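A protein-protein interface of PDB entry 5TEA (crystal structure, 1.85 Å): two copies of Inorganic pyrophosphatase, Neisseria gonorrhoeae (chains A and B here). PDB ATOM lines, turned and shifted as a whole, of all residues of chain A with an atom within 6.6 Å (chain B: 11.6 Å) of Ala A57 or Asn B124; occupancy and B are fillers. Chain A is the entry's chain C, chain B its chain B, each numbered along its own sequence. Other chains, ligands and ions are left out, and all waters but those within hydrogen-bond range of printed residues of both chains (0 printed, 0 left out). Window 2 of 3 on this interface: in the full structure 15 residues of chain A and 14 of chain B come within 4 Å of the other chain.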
ATOM      1  N   GLY A  35     -33.404  -7.945  -3.873  1.00  0.00           N
ATOM      2  CA  GLY A  35     -33.332  -6.504  -3.942  1.00  0.00           C
ATOM      3  C   GLY A  35     -32.183  -5.874  -3.194  1.00  0.00           C
ATOM      4  O   GLY A  35     -32.026  -4.645  -3.261  1.00  0.00           O
ATOM      5  N   ASN A  37     -28.144  -5.098  -2.400  1.00  0.00           N
ATOM      6  CA  ASN A  37     -26.801  -5.076  -2.979  1.00  0.00           C
ATOM      7  C   ASN A  37     -25.730  -5.364  -1.929  1.00  0.00           C
ATOM      8  O   ASN A  37     -24.571  -4.946  -2.081  1.00  0.00           O
ATOM      9  CB  ASN A  37     -26.519  -3.733  -3.683  1.00  0.00           C
ATOM     10  CG  ASN A  37     -26.378  -2.563  -2.711  1.00  0.00           C
ATOM     11  OD1 ASN A  37     -27.011  -2.525  -1.653  1.00  0.00           O
ATOM     12  ND2 ASN A  37     -25.538  -1.595  -3.074  1.00  0.00           N
ATOM     13  N   ILE A  54     -20.035  -4.622  -0.419  1.00  0.00           N
ATOM     14  CA  ILE A  54     -21.158  -3.925  -1.034  1.00  0.00           C
ATOM     15  C   ILE A  54     -21.006  -4.046  -2.541  1.00  0.00           C
ATOM     16  O   ILE A  54     -19.928  -3.772  -3.080  1.00  0.00           O
ATOM     17  CB  ILE A  54     -21.185  -2.439  -0.628  1.00  0.00           C
ATOM     18  CG1 ILE A  54     -21.049  -2.275   0.892  1.00  0.00           C
ATOM     19  CG2 ILE A  54     -22.429  -1.757  -1.233  1.00  0.00           C
ATOM     20  CD1 ILE A  54     -22.248  -2.778   1.713  1.00  0.00           C
ATOM     21  N   GLU A  55     -22.098  -4.464  -3.231  1.00  0.00           N
ATOM     22  CA  GLU A  55     -22.142  -4.552  -4.680  1.00  0.00           C
ATOM     23  C   GLU A  55     -22.695  -3.258  -5.263  1.00  0.00           C
ATOM     24  O   GLU A  55     -23.366  -2.500  -4.562  1.00  0.00           O
ATOM     25  CB  GLU A  55     -23.034  -5.723  -5.108  1.00  0.00           C
ATOM     26  CG  GLU A  55     -22.662  -7.075  -4.514  1.00  0.00           C
ATOM     27  CD  GLU A  55     -21.526  -7.735  -5.241  1.00  0.00           C
ATOM     28  OE1 GLU A  55     -20.821  -7.039  -6.010  1.00  0.00           O
ATOM     29  OE2 GLU A  55     -21.357  -8.963  -5.072  1.00  0.00           O
ATOM     30  N   PRO A  56     -22.422  -2.973  -6.541  1.00  0.00           N
ATOM     31  CA  PRO A  56     -23.097  -1.853  -7.203  1.00  0.00           C
ATOM     32  C   PRO A  56     -24.604  -1.969  -7.023  1.00  0.00           C
ATOM     33  O   PRO A  56     -25.190  -3.044  -7.190  1.00  0.00           O
ATOM     34  CB  PRO A  56     -22.703  -2.016  -8.682  1.00  0.00           C
ATOM     35  CG  PRO A  56     -21.445  -2.857  -8.671  1.00  0.00           C
ATOM     36  CD  PRO A  56     -21.604  -3.765  -7.485  1.00  0.00           C
ATOM     37  N   ALA A  57     -25.229  -0.840  -6.703  1.00  0.00           N
ATOM     38  CA  ALA A  57     -26.670  -0.814  -6.494  1.00  0.00           C
ATOM     39  C   ALA A  57     -27.441  -1.220  -7.745  1.00  0.00           C
ATOM     40  O   ALA A  57     -28.540  -1.777  -7.638  1.00  0.00           O
ATOM     41  CB  ALA A  57     -27.096   0.582  -6.023  1.00  0.00           C
ATOM     42  N   ILE A  58     -26.891  -0.972  -8.937  1.00  0.00           N
ATOM     43  CA  ILE A  58     -27.572  -1.425 -10.148  1.00  0.00           C
ATOM     44  C   ILE A  58     -27.606  -2.943 -10.276  1.00  0.00           C
ATOM     45  O   ILE A  58     -28.373  -3.467 -11.088  1.00  0.00           O
ATOM     46  CB  ILE A  58     -26.925  -0.812 -11.401  1.00  0.00           C
ATOM     47  CG1 ILE A  58     -25.425  -1.140 -11.448  1.00  0.00           C
ATOM     48  CG2 ILE A  58     -27.155   0.701 -11.434  1.00  0.00           C
ATOM     49  CD1 ILE A  58     -24.821  -0.969 -12.840  1.00  0.00           C
ATOM     50  N   PHE A  59     -26.827  -3.662  -9.473  1.00  0.00           N
ATOM     51  CA  PHE A  59     -26.795  -5.120  -9.472  1.00  0.00           C
ATOM     52  C   PHE A  59     -27.329  -5.686  -8.159  1.00  0.00           C
ATOM     53  O   PHE A  59     -26.818  -6.680  -7.646  1.00  0.00           O
ATOM     54  CB  PHE A  59     -25.375  -5.629  -9.731  1.00  0.00           C
ATOM     55  CG  PHE A  59     -24.841  -5.247 -11.072  1.00  0.00           C
ATOM     56  CD1 PHE A  59     -25.658  -5.289 -12.179  1.00  0.00           C
ATOM     57  CD2 PHE A  59     -23.530  -4.797 -11.218  1.00  0.00           C
ATOM     58  CE1 PHE A  59     -25.176  -4.920 -13.425  1.00  0.00           C
ATOM     59  CE2 PHE A  59     -23.050  -4.424 -12.452  1.00  0.00           C
ATOM     60  CZ  PHE A  59     -23.878  -4.491 -13.562  1.00  0.00           C
ATOM     61  N   ALA A  60     -28.379  -5.071  -7.614  1.00  0.00           N
ATOM     62  CA  ALA A  60     -29.104  -5.698  -6.522  1.00  0.00           C
ATOM     63  C   ALA A  60     -29.589  -7.079  -6.963  1.00  0.00           C
ATOM     64  O   ALA A  60     -29.908  -7.305  -8.137  1.00  0.00           O
ATOM     65  CB  ALA A  60     -30.277  -4.816  -6.092  1.00  0.00           C
ATOM     66  N   LYS A  61     -29.584  -8.017  -6.024  1.00  0.00           N
ATOM     67  CA  LYS A  61     -29.917  -9.405  -6.336  1.00  0.00           C
ATOM     68  C   LYS A  61     -31.346  -9.509  -6.862  1.00  0.00           C
ATOM     69  O   LYS A  61     -32.269  -8.965  -6.243  1.00  0.00           O
ATOM     70  CB  LYS A  61     -29.753 -10.294  -5.095  1.00  0.00           C
ATOM     71  CG  LYS A  61     -28.292 -10.596  -4.721  1.00  0.00           C
ATOM     72  CD  LYS A  61     -27.572 -11.293  -5.876  1.00  0.00           C
ATOM     73  CE  LYS A  61     -26.053 -11.141  -5.800  1.00  0.00           C
ATOM     74  NZ  LYS A  61     -25.379 -11.400  -7.130  1.00  0.00           N
ATOM     75  N   ASN B  64     -25.349   3.144  10.454  1.00  0.00           N
ATOM     76  CA  ASN B  64     -25.447   1.856  11.127  1.00  0.00           C
ATOM     77  C   ASN B  64     -24.626   1.924  12.407  1.00  0.00           C
ATOM     78  O   ASN B  64     -23.681   2.713  12.517  1.00  0.00           O
ATOM     79  CB  ASN B  64     -24.951   0.723  10.226  1.00  0.00           C
ATOM     80  CG  ASN B  64     -25.632   0.716   8.883  1.00  0.00           C
ATOM     81  OD1 ASN B  64     -26.800   0.305   8.759  1.00  0.00           O
ATOM     82  ND2 ASN B  64     -24.911   1.154   7.857  1.00  0.00           N
ATOM     83  N   VAL B  84     -20.824   3.596   8.085  1.00  0.00           N
ATOM     84  CA  VAL B  84     -21.508   4.426   7.098  1.00  0.00           C
ATOM     85  C   VAL B  84     -21.682   3.628   5.810  1.00  0.00           C
ATOM     86  O   VAL B  84     -20.708   3.140   5.236  1.00  0.00           O
ATOM     87  CB  VAL B  84     -20.735   5.728   6.843  1.00  0.00           C
ATOM     88  CG1 VAL B  84     -21.389   6.550   5.726  1.00  0.00           C
ATOM     89  CG2 VAL B  84     -20.617   6.533   8.160  1.00  0.00           C
ATOM     90  N   THR B  85     -22.928   3.486   5.363  1.00  0.00           N
ATOM     91  CA  THR B  85     -23.252   2.849   4.095  1.00  0.00           C
ATOM     92  C   THR B  85     -24.340   3.665   3.413  1.00  0.00           C
ATOM     93  O   THR B  85     -25.041   4.451   4.051  1.00  0.00           O
ATOM     94  CB  THR B  85     -23.774   1.402   4.255  1.00  0.00           C
ATOM     95  OG1 THR B  85     -24.964   1.412   5.052  1.00  0.00           O
ATOM     96  CG2 THR B  85     -22.738   0.472   4.896  1.00  0.00           C
ATOM     97  N   GLU B  86     -24.515   3.430   2.114  1.00  0.00           N
ATOM     98  CA  GLU B  86     -25.615   4.080   1.401  1.00  0.00           C
ATOM     99  C   GLU B  86     -26.965   3.474   1.784  1.00  0.00           C
ATOM    100  O   GLU B  86     -27.956   4.201   1.941  1.00  0.00           O
ATOM    101  CB  GLU B  86     -25.387   3.993  -0.115  1.00  0.00           C
ATOM    102  CG  GLU B  86     -24.405   5.034  -0.683  1.00  0.00           C
ATOM    103  CD  GLU B  86     -22.928   4.589  -0.710  1.00  0.00           C
ATOM    104  OE1 GLU B  86     -22.624   3.418  -1.067  1.00  0.00           O
ATOM    105  OE2 GLU B  86     -22.062   5.439  -0.386  1.00  0.00           O
ATOM    106  N   GLN B  87     -27.031   2.149   1.936  1.00  0.00           N
ATOM    107  CA  GLN B  87     -28.252   1.470   2.315  1.00  0.00           C
ATOM    108  C   GLN B  87     -28.075   0.758   3.658  1.00  0.00           C
ATOM    109  O   GLN B  87     -27.003   0.205   3.929  1.00  0.00           O
ATOM    110  CB  GLN B  87     -28.663   0.468   1.218  1.00  0.00           C
ATOM    111  CG  GLN B  87     -29.071   1.137  -0.116  1.00  0.00           C
ATOM    112  CD  GLN B  87     -27.910   1.368  -1.089  1.00  0.00           C
ATOM    113  OE1 GLN B  87     -26.877   0.694  -1.029  1.00  0.00           O
ATOM    114  NE2 GLN B  87     -28.091   2.318  -2.008  1.00  0.00           N
ATOM    115  N   PRO B  88     -29.093   0.760   4.518  1.00  0.00           N
ATOM    116  CA  PRO B  88     -28.915   0.195   5.870  1.00  0.00           C
ATOM    117  C   PRO B  88     -28.505  -1.274   5.865  1.00  0.00           C
ATOM    118  O   PRO B  88     -28.928  -2.067   5.016  1.00  0.00           O
ATOM    119  CB  PRO B  88     -30.296   0.385   6.523  1.00  0.00           C
ATOM    120  CG  PRO B  88     -30.931   1.496   5.767  1.00  0.00           C
ATOM    121  CD  PRO B  88     -30.417   1.390   4.349  1.00  0.00           C
ATOM    122  N   VAL B 118     -16.214   2.294   7.307  1.00  0.00           N
ATOM    123  CA  VAL B 118     -16.975   1.922   6.113  1.00  0.00           C
ATOM    124  C   VAL B 118     -16.641   0.470   5.795  1.00  0.00           C
ATOM    125  O   VAL B 118     -15.600  -0.047   6.231  1.00  0.00           O
ATOM    126  CB  VAL B 118     -16.640   2.839   4.911  1.00  0.00           C
ATOM    127  CG1 VAL B 118     -17.103   4.282   5.198  1.00  0.00           C
ATOM    128  CG2 VAL B 118     -15.118   2.801   4.614  1.00  0.00           C
ATOM    129  N   PRO B 119     -17.488  -0.217   5.034  1.00  0.00           N
ATOM    130  CA  PRO B 119     -17.119  -1.570   4.596  1.00  0.00           C
ATOM    131  C   PRO B 119     -15.787  -1.532   3.861  1.00  0.00           C
ATOM    132  O   PRO B 119     -15.504  -0.596   3.104  1.00  0.00           O
ATOM    133  CB  PRO B 119     -18.263  -1.970   3.655  1.00  0.00           C
ATOM    134  CG  PRO B 119     -19.419  -1.085   4.069  1.00  0.00           C
ATOM    135  CD  PRO B 119     -18.767   0.219   4.443  1.00  0.00           C
ATOM    136  N   ALA B 120     -14.959  -2.552   4.106  1.00  0.00           N
ATOM    137  CA  ALA B 120     -13.611  -2.545   3.533  1.00  0.00           C
ATOM    138  C   ALA B 120     -13.635  -2.754   2.023  1.00  0.00           C
ATOM    139  O   ALA B 120     -12.721  -2.307   1.325  1.00  0.00           O
ATOM    140  CB  ALA B 120     -12.735  -3.611   4.194  1.00  0.00           C
ATOM    141  N   ASP B 121     -14.675  -3.400   1.508  1.00  0.00           N
ATOM    142  CA  ASP B 121     -14.825  -3.694   0.081  1.00  0.00           C
ATOM    143  C   ASP B 121     -16.194  -3.128  -0.314  1.00  0.00           C
ATOM    144  O   ASP B 121     -17.214  -3.797  -0.151  1.00  0.00           O
ATOM    145  CB  ASP B 121     -14.707  -5.212  -0.147  1.00  0.00           C
ATOM    146  CG  ASP B 121     -14.682  -5.607  -1.618  1.00  0.00           C
ATOM    147  OD1 ASP B 121     -14.937  -4.759  -2.493  1.00  0.00           O
ATOM    148  OD2 ASP B 121     -14.414  -6.794  -1.891  1.00  0.00           O
ATOM    149  N   ASP B 122     -16.215  -1.888  -0.801  1.00  0.00           N
ATOM    150  CA  ASP B 122     -17.451  -1.205  -1.204  1.00  0.00           C
ATOM    151  C   ASP B 122     -17.397  -0.955  -2.708  1.00  0.00           C
ATOM    152  O   ASP B 122     -16.778   0.013  -3.160  1.00  0.00           O
ATOM    153  CB  ASP B 122     -17.627   0.109  -0.437  1.00  0.00           C
ATOM    154  CG  ASP B 122     -18.978   0.780  -0.723  1.00  0.00           C
ATOM    155  OD1 ASP B 122     -19.578   0.538  -1.789  1.00  0.00           O
ATOM    156  OD2 ASP B 122     -19.456   1.543   0.124  1.00  0.00           O
ATOM    157  N   ARG B 123     -18.062  -1.813  -3.483  1.00  0.00           N
ATOM    158  CA  ARG B 123     -18.065  -1.660  -4.930  1.00  0.00           C
ATOM    159  C   ARG B 123     -19.245  -0.841  -5.420  1.00  0.00           C
ATOM    160  O   ARG B 123     -19.459  -0.752  -6.635  1.00  0.00           O
ATOM    161  CB  ARG B 123     -18.027  -3.040  -5.600  1.00  0.00           C
ATOM    162  CG  ARG B 123     -16.791  -3.816  -5.136  1.00  0.00           C
ATOM    163  CD  ARG B 123     -16.528  -5.103  -5.873  1.00  0.00           C
ATOM    164  NE  ARG B 123     -15.573  -5.904  -5.105  1.00  0.00           N
ATOM    165  CZ  ARG B 123     -15.127  -7.105  -5.464  1.00  0.00           C
ATOM    166  NH1 ARG B 123     -15.539  -7.666  -6.596  1.00  0.00           N
ATOM    167  NH2 ARG B 123     -14.273  -7.750  -4.676  1.00  0.00           N
ATOM    168  N   ASN B 124     -20.012  -0.242  -4.506  1.00  0.00           N
ATOM    169  CA  ASN B 124     -21.033   0.708  -4.929  1.00  0.00           C
ATOM    170  C   ASN B 124     -20.463   2.116  -5.086  1.00  0.00           C
ATOM    171  O   ASN B 124     -20.763   2.803  -6.066  1.00  0.00           O
ATOM    172  CB  ASN B 124     -22.193   0.732  -3.932  1.00  0.00           C
ATOM    173  CG  ASN B 124     -23.322   1.649  -4.374  1.00  0.00           C
ATOM    174  OD1 ASN B 124     -23.846   1.527  -5.484  1.00  0.00           O
ATOM    175  ND2 ASN B 124     -23.697   2.582  -3.507  1.00  0.00           N
ATOM    176  N   ASN B 125     -19.659   2.579  -4.133  1.00  0.00           N
ATOM    177  CA  ASN B 125     -18.983   3.857  -4.307  1.00  0.00           C
ATOM    178  C   ASN B 125     -17.516   3.695  -4.691  1.00  0.00           C
ATOM    179  O   ASN B 125     -16.813   4.698  -4.839  1.00  0.00           O
ATOM    180  CB  ASN B 125     -19.128   4.728  -3.049  1.00  0.00           C
ATOM    181  CG  ASN B 125     -18.445   4.140  -1.811  1.00  0.00           C
ATOM    182  OD1 ASN B 125     -17.458   3.424  -1.902  1.00  0.00           O
ATOM    183  ND2 ASN B 125     -18.996   4.438  -0.649  1.00  0.00           N
ATOM    184  N   GLY B 126     -17.050   2.468  -4.888  1.00  0.00           N
ATOM    185  CA  GLY B 126     -15.670   2.284  -5.308  1.00  0.00           C
ATOM    186  C   GLY B 126     -14.654   2.634  -4.242  1.00  0.00           C
ATOM    187  O   GLY B 126     -13.586   3.168  -4.563  1.00  0.00           O
ATOM    188  N   ASN B 127     -14.955   2.326  -2.976  1.00  0.00           N
ATOM    189  CA  ASN B 127     -14.080   2.644  -1.848  1.00  0.00           C
ATOM    190  C   ASN B 127     -13.731   4.131  -1.826  1.00  0.00           C
ATOM    191  O   ASN B 127     -12.575   4.524  -1.664  1.00  0.00           O
ATOM    192  CB  ASN B 127     -12.824   1.773  -1.885  1.00  0.00           C
ATOM    193  CG  ASN B 127     -13.169   0.299  -1.909  1.00  0.00           C
ATOM    194  OD1 ASN B 127     -13.891  -0.180  -1.038  1.00  0.00           O
ATOM    195  ND2 ASN B 127     -12.693  -0.418  -2.924  1.00  0.00           N
ATOM    196  N   ALA B 128     -14.759   4.963  -1.990  1.00  0.00           N
ATOM    197  CA  ALA B 128     -14.564   6.409  -2.076  1.00  0.00           C
ATOM    198  C   ALA B 128     -14.117   7.037  -0.760  1.00  0.00           C
ATOM    199  O   ALA B 128     -13.598   8.159  -0.769  1.00  0.00           O
ATOM    200  CB  ALA B 128     -15.866   7.085  -2.520  1.00  0.00           C
ATOM    201  N   TYR B 129     -14.332   6.375   0.366  1.00  0.00           N
ATOM    202  CA  TYR B 129     -14.162   6.994   1.679  1.00  0.00           C
ATOM    203  C   TYR B 129     -13.033   6.304   2.428  1.00  0.00           C
ATOM    204  O   TYR B 129     -13.181   5.164   2.879  1.00  0.00           O
ATOM    205  CB  TYR B 129     -15.459   6.919   2.475  1.00  0.00           C
ATOM    206  CG  TYR B 129     -16.628   7.544   1.758  1.00  0.00           C
ATOM    207  CD1 TYR B 129     -16.507   8.782   1.140  1.00  0.00           C
ATOM    208  CD2 TYR B 129     -17.850   6.892   1.697  1.00  0.00           C
ATOM    209  CE1 TYR B 129     -17.586   9.361   0.479  1.00  0.00           C
ATOM    210  CE2 TYR B 129     -18.931   7.463   1.042  1.00  0.00           C
ATOM    211  CZ  TYR B 129     -18.788   8.696   0.433  1.00  0.00           C
ATOM    212  OH  TYR B 129     -19.856   9.260  -0.233  1.00  0.00           O
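The side-chain amide oxygen of Gln B87 sits close to the side-chain amide oxygen of Asn A37 (3.3 Å). The backbone carbonyl oxygen (O) of Asp B121 lies within hydrogen-bond range of the backbone NH (N) of Ile A54, 3.0 Å away. The backbone NH (N) of Arg B123 is in hydrogen-bond range of the backbone carbonyl oxygen (O) of Ile A54 (2.7 Å). The side-chain amide oxygen of Asn B124 lies within hydrogen-bond range of the backbone NH of Ala A57, at 3.0 Å.
O of Gln B87 lies within hydrogen-bond range of OG1 of Thr B85. The side-chain amide nitrogen (ND2) of Asn B124 lies within hydrogen-bond range of the side-chain carboxylate (OE1) of Glu B86 (2.8 Å). The side-chain carboxylate (OD1) of Asp B121 lies within salt-bridge range of the guanidinium group (NE) of Arg B123 (2.9 Å). The backbone NH of Asn B124 sits at hydrogen-bond distance from the side-chain carboxylate of Asp B122 (2.9 Å). OD2 of Asp B122 sits at hydrogen-bond distance from ND2 of Asn B125. The side-chain amide oxygen (OD1) of Asn B127 is in hydrogen-bond range of the backbone NH (N) of Asp B122, 2.9 Å away.
Ile A54 touches Pro B119 (CG1 to CG, 3.8 Å). CB of Ile A54 touches OD1 of Asp B122, 3.6 Å away. Ile A54 touches Asn B124. CB of Asn B124 touches O of Glu A55, 3.5 Å away. Pro A56 touches Arg B123. CA of Pro A56 touches OD1 of Asn B124, at 3.9 Å.
Of chain B, only Asn B124 (3.0 Å) comes within 4 Å of Ala A57. Of chain A, only Ile A54 (3.7 Å), Glu A55 (3.5 Å), Pro A56 (3.9 Å) and Ala A57 (3.0 Å) come within 4 Å of Asn B124. Ile A54 touches five residues of chain B. No residue of chain B comes within 4 Å of Ala A60. Of the printed residues of chain B, Glu A55 touches Asn B124. Of the printed residues of chain A, Arg B123 touches Ile A54 (2.7 Å) and Pro A56 (3.5 Å). Printed residues of chain B within 4 Å of Asn A37: Gln B87. The nearest residue of chain A that does not touch Asn B124 is Asn A37 (4.1 Å).
Printed residues of chain B that touch a printed residue of chain A: Gln B87, Pro B119, Asp B121, Asp B122, Arg B123 and Asn B124. Hydrophobic or aromatic side chains of chain B that line the printed part of chain A: Pro B119.
No position is printed for both chains.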
